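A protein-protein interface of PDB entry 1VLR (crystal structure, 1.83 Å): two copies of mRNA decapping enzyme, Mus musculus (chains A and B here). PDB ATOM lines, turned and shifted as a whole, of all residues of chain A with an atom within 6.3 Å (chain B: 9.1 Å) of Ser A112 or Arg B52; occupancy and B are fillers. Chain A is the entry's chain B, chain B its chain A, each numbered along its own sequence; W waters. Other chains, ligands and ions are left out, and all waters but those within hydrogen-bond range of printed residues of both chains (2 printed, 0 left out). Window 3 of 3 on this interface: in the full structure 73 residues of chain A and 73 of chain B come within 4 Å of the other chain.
Water W1 bridges O of Pro A113 and O of Val B51.
Water W2 lies within hydrogen-bond range of the backbone carbonyl oxygen (O) of Val B51, the backbone carbonyl oxygen (O) of Pro A113 and the backbone NH (N) of Leu A115.
No residue of chain B comes within 4 Å of Gly A111.
No residue of chain B comes within 4 Å of Pro A113.
Of the printed residues of chain A, Val B142 touches Tyr A127 (3.8 Å).
Of the printed residues of chain B, Leu A109 touches Leu B53 (3.6 Å).
Of the printed residues of chain A, Val B51 touches Leu A115 (3.4 Å) and Tyr A127 (3.98 Å).
Of the printed residues of chain A, Pro B54 touches Tyr A127 (3.5 Å).
Glu A114 touches none of the printed residues of chain B.
Pro B50 touches none of the printed residues of chain A.
Of the 9 printed residues of chain A, 4 touch a printed residue of chain B.
Printed residues of chain A that touch a printed residue of chain B: Leu A109, Ser A112, Leu A115 and Tyr A127.
Hydrophobic or aromatic side chains of chain A within 4 Å of the printed part of chain B: Leu A115 and Tyr A127.
Of the 9 printed residues of chain B, 5 touch a printed residue of chain A.
Among the printed residues, no Asp or Glu carboxylate lies within 4 Å of a Lys or Arg side-chain nitrogen of the other chain.
No position is printed for both chains.
The guanidinium group of Arg B52 sits at hydrogen-bond distance from the side-chain hydroxyl of Ser A112.
The backbone carbonyl oxygen (O) of Arg B52 lies within hydrogen-bond range of the side-chain hydroxyl (OH) of Tyr A127, at 3.4 Å.
CD1 of Leu B53 touches O of Leu A109, at 3.6 Å.
Leu A115 touches Val B51 (O to CB, 3.4 Å).
Leu A115 touches Arg B52.
Leu A115 touches Leu B53 (CD1 to N, 3.8 Å).
CE2 of Tyr A127 touches CG1 of Val B51, 3.98 Å away.
Tyr A127 touches Pro B54.
Tyr A127 touches Val B142 (CE1 to CG2, 3.8 Å).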
ATOM      1  N   LEU A 109      20.182   8.894   9.047  1.00  0.00           N
ATOM      2  CA  LEU A 109      20.790   9.385   7.820  1.00  0.00           C
ATOM      3  C   LEU A 109      22.133  10.033   7.988  1.00  0.00           C
ATOM      4  O   LEU A 109      22.799  10.356   6.993  1.00  0.00           O
ATOM      5  CB  LEU A 109      19.866  10.414   7.200  1.00  0.00           C
ATOM      6  CG  LEU A 109      18.578   9.854   6.614  1.00  0.00           C
ATOM      7  CD1 LEU A 109      17.669  11.010   6.266  1.00  0.00           C
ATOM      8  CD2 LEU A 109      18.859   9.017   5.419  1.00  0.00           C
ATOM      9  N   THR A 110      22.491  10.310   9.231  1.00  0.00           N
ATOM     10  CA  THR A 110      23.735  10.979   9.484  1.00  0.00           C
ATOM     11  C   THR A 110      24.745   9.989   9.908  1.00  0.00           C
ATOM     12  O   THR A 110      24.458   8.809  10.229  1.00  0.00           O
ATOM     13  CB  THR A 110      23.635  12.060  10.531  1.00  0.00           C
ATOM     14  OG1 THR A 110      23.085  11.537  11.744  1.00  0.00           O
ATOM     15  CG2 THR A 110      22.714  13.168  10.068  1.00  0.00           C
ATOM     16  N   GLY A 111      25.959  10.511   9.932  1.00  0.00           N
ATOM     17  CA  GLY A 111      27.107   9.721  10.173  1.00  0.00           C
ATOM     18  C   GLY A 111      27.335   9.081   8.839  1.00  0.00           C
ATOM     19  O   GLY A 111      27.301   9.758   7.764  1.00  0.00           O
ATOM     20  N   SER A 112      27.559   7.780   8.935  1.00  0.00           N
ATOM     21  CA  SER A 112      27.882   6.956   7.820  1.00  0.00           C
ATOM     22  C   SER A 112      26.921   5.770   7.907  1.00  0.00           C
ATOM     23  O   SER A 112      27.284   4.674   8.340  1.00  0.00           O
ATOM     24  CB  SER A 112      29.347   6.544   7.894  1.00  0.00           C
ATOM     25  OG  SER A 112      30.166   7.728   7.910  1.00  0.00           O
ATOM     26  N   PRO A 113      25.673   6.018   7.513  1.00  0.00           N
ATOM     27  CA  PRO A 113      24.679   4.958   7.463  1.00  0.00           C
ATOM     28  C   PRO A 113      25.095   3.893   6.465  1.00  0.00           C
ATOM     29  O   PRO A 113      25.746   4.168   5.444  1.00  0.00           O
ATOM     30  CB  PRO A 113      23.419   5.689   6.970  1.00  0.00           C
ATOM     31  CG  PRO A 113      23.936   6.883   6.241  1.00  0.00           C
ATOM     32  CD  PRO A 113      25.108   7.305   7.049  1.00  0.00           C
ATOM     33  N   GLU A 114      24.702   2.667   6.749  1.00  0.00           N
ATOM     34  CA  GLU A 114      25.007   1.556   5.893  1.00  0.00           C
ATOM     35  C   GLU A 114      24.050   1.555   4.728  1.00  0.00           C
ATOM     36  O   GLU A 114      22.822   1.413   4.899  1.00  0.00           O
ATOM     37  CB  GLU A 114      24.926   0.221   6.673  1.00  0.00           C
ATOM     38  CG  GLU A 114      25.265  -0.960   5.776  1.00  0.00           C
ATOM     39  CD  GLU A 114      25.144  -2.346   6.432  1.00  0.00           C
ATOM     40  OE1 GLU A 114      24.949  -2.425   7.641  1.00  0.00           O
ATOM     41  OE2 GLU A 114      25.256  -3.360   5.700  1.00  0.00           O
ATOM     42  N   LEU A 115      24.593   1.689   3.529  1.00  0.00           N
ATOM     43  CA  LEU A 115      23.785   1.874   2.344  1.00  0.00           C
ATOM     44  C   LEU A 115      24.212   0.975   1.227  1.00  0.00           C
ATOM     45  O   LEU A 115      25.377   0.619   1.134  1.00  0.00           O
ATOM     46  CB  LEU A 115      23.932   3.312   1.829  1.00  0.00           C
ATOM     47  CG  LEU A 115      23.510   4.429   2.782  1.00  0.00           C
ATOM     48  CD1 LEU A 115      24.183   5.683   2.357  1.00  0.00           C
ATOM     49  CD2 LEU A 115      21.965   4.584   2.783  1.00  0.00           C
ATOM     50  N   LEU A 117      23.520   1.262  -2.947  1.00  0.00           N
ATOM     51  CA  LEU A 117      22.906   2.065  -3.990  1.00  0.00           C
ATOM     52  C   LEU A 117      22.167   1.147  -4.928  1.00  0.00           C
ATOM     53  O   LEU A 117      22.692   0.103  -5.299  1.00  0.00           O
ATOM     54  CB  LEU A 117      23.943   2.855  -4.754  1.00  0.00           C
ATOM     55  CG  LEU A 117      23.415   3.719  -5.881  1.00  0.00           C
ATOM     56  CD1 LEU A 117      22.799   4.966  -5.313  1.00  0.00           C
ATOM     57  CD2 LEU A 117      24.520   4.043  -6.918  1.00  0.00           C
ATOM     58  N   TYR A 127      18.337   4.049  -2.463  1.00  0.00           N
ATOM     59  CA  TYR A 127      19.199   3.170  -1.738  1.00  0.00           C
ATOM     60  C   TYR A 127      18.379   2.196  -0.940  1.00  0.00           C
ATOM     61  O   TYR A 127      17.190   2.432  -0.688  1.00  0.00           O
ATOM     62  CB  TYR A 127      20.028   3.945  -0.736  1.00  0.00           C
ATOM     63  CG  TYR A 127      20.909   5.011  -1.338  1.00  0.00           C
ATOM     64  CD1 TYR A 127      20.379   6.219  -1.785  1.00  0.00           C
ATOM     65  CD2 TYR A 127      22.294   4.807  -1.450  1.00  0.00           C
ATOM     66  CE1 TYR A 127      21.217   7.204  -2.329  1.00  0.00           C
ATOM     67  CE2 TYR A 127      23.119   5.779  -1.979  1.00  0.00           C
ATOM     68  CZ  TYR A 127      22.578   6.955  -2.428  1.00  0.00           C
ATOM     69  OH  TYR A 127      23.417   7.927  -2.939  1.00  0.00           O
ATOM     70  N   PRO B  50      33.010   2.485   0.642  1.00  0.00           N
ATOM     71  CA  PRO B  50      31.947   2.989   1.519  1.00  0.00           C
ATOM     72  C   PRO B  50      30.898   3.768   0.729  1.00  0.00           C
ATOM     73  O   PRO B  50      31.213   4.828   0.184  1.00  0.00           O
ATOM     74  CB  PRO B  50      32.694   3.925   2.499  1.00  0.00           C
ATOM     75  CG  PRO B  50      34.178   3.703   2.229  1.00  0.00           C
ATOM     76  CD  PRO B  50      34.252   3.259   0.796  1.00  0.00           C
ATOM     77  N   VAL B  51      29.674   3.241   0.673  1.00  0.00           N
ATOM     78  CA  VAL B  51      28.583   3.860  -0.064  1.00  0.00           C
ATOM     79  C   VAL B  51      28.058   5.001   0.774  1.00  0.00           C
ATOM     80  O   VAL B  51      27.789   4.848   1.962  1.00  0.00           O
ATOM     81  CB  VAL B  51      27.462   2.852  -0.381  1.00  0.00           C
ATOM     82  CG1 VAL B  51      26.299   3.534  -1.128  1.00  0.00           C
ATOM     83  CG2 VAL B  51      28.016   1.695  -1.215  1.00  0.00           C
ATOM     84  N   ARG B  52      27.987   6.179   0.169  1.00  0.00           N
ATOM     85  CA  ARG B  52      27.560   7.352   0.864  1.00  0.00           C
ATOM     86  C   ARG B  52      26.419   8.057   0.134  1.00  0.00           C
ATOM     87  O   ARG B  52      26.246   7.919  -1.076  1.00  0.00           O
ATOM     88  CB  ARG B  52      28.700   8.352   0.970  1.00  0.00           C
ATOM     89  CG  ARG B  52      29.982   7.811   1.546  1.00  0.00           C
ATOM     90  CD  ARG B  52      30.270   8.348   2.872  1.00  0.00           C
ATOM     91  NE  ARG B  52      31.307   7.565   3.540  1.00  0.00           N
ATOM     92  CZ  ARG B  52      31.617   7.707   4.818  1.00  0.00           C
ATOM     93  NH1 ARG B  52      30.979   8.624   5.563  1.00  0.00           N
ATOM     94  NH2 ARG B  52      32.588   6.953   5.344  1.00  0.00           N
ATOM     95  N   LEU B  53      25.671   8.816   0.914  1.00  0.00           N
ATOM     96  CA  LEU B  53      24.735   9.779   0.404  1.00  0.00           C
ATOM     97  C   LEU B  53      25.554  10.858  -0.325  1.00  0.00           C
ATOM     98  O   LEU B  53      26.742  11.074   0.014  1.00  0.00           O
ATOM     99  CB  LEU B  53      23.954  10.392   1.558  1.00  0.00           C
ATOM    100  CG  LEU B  53      22.970   9.436   2.287  1.00  0.00           C
ATOM    101  CD1 LEU B  53      22.330  10.182   3.447  1.00  0.00           C
ATOM    102  CD2 LEU B  53      21.934   8.874   1.361  1.00  0.00           C
ATOM    103  N   PRO B  54      24.965  11.496  -1.338  1.00  0.00           N
ATOM    104  CA  PRO B  54      25.681  12.518  -2.112  1.00  0.00           C
ATOM    105  C   PRO B  54      25.839  13.898  -1.433  1.00  0.00           C
ATOM    106  O   PRO B  54      25.873  14.931  -2.112  1.00  0.00           O
ATOM    107  CB  PRO B  54      24.827  12.615  -3.362  1.00  0.00           C
ATOM    108  CG  PRO B  54      23.422  12.388  -2.877  1.00  0.00           C
ATOM    109  CD  PRO B  54      23.618  11.239  -1.881  1.00  0.00           C
ATOM    110  N   PHE B  55      25.866  13.941  -0.114  1.00  0.00           N
ATOM    111  CA  PHE B  55      25.982  15.180   0.621  1.00  0.00           C
ATOM    112  C   PHE B  55      26.473  14.891   2.030  1.00  0.00           C
ATOM    113  O   PHE B  55      26.585  13.736   2.433  1.00  0.00           O
ATOM    114  CB  PHE B  55      24.666  15.943   0.663  1.00  0.00           C
ATOM    115  CG  PHE B  55      23.490  15.098   1.044  1.00  0.00           C
ATOM    116  CD1 PHE B  55      23.315  14.683   2.359  1.00  0.00           C
ATOM    117  CD2 PHE B  55      22.557  14.737   0.096  1.00  0.00           C
ATOM    118  CE1 PHE B  55      22.257  13.886   2.691  1.00  0.00           C
ATOM    119  CE2 PHE B  55      21.491  13.958   0.435  1.00  0.00           C
ATOM    120  CZ  PHE B  55      21.351  13.520   1.725  1.00  0.00           C
ATOM    121  N   SER B  56      26.778  15.952   2.762  1.00  0.00           N
ATOM    122  CA  SER B  56      27.304  15.826   4.139  1.00  0.00           C
ATOM    123  C   SER B  56      26.307  16.219   5.156  1.00  0.00           C
ATOM    124  O   SER B  56      25.785  17.308   5.107  1.00  0.00           O
ATOM    125  CB  SER B  56      28.543  16.692   4.312  1.00  0.00           C
ATOM    126  OG  SER B  56      29.596  16.156   3.523  1.00  0.00           O
ATOM    127  N   GLY B  57      26.038  15.328   6.095  1.00  0.00           N
ATOM    128  CA  GLY B  57      25.152  15.653   7.185  1.00  0.00           C
ATOM    129  C   GLY B  57      23.693  15.612   6.708  1.00  0.00           C
ATOM    130  O   GLY B  57      23.413  15.415   5.516  1.00  0.00           O
ATOM    131  N   VAL B 142      16.446   9.625  -2.543  1.00  0.00           N
ATOM    132  CA  VAL B 142      17.129  10.879  -2.339  1.00  0.00           C
ATOM    133  C   VAL B 142      16.982  11.808  -3.578  1.00  0.00           C
ATOM    134  O   VAL B 142      17.230  11.396  -4.722  1.00  0.00           O
ATOM    135  CB  VAL B 142      18.605  10.628  -2.028  1.00  0.00           C
ATOM    136  CG1 VAL B 142      19.321  11.967  -1.810  1.00  0.00           C
ATOM    137  CG2 VAL B 142      18.763   9.733  -0.782  1.00  0.00           C
HETATM  138  O   HOH W   1      27.263   6.203   4.568  1.00  0.00           O
HETATM  139  O   HOH W   2      27.421   2.631   3.698  1.00  0.00           O
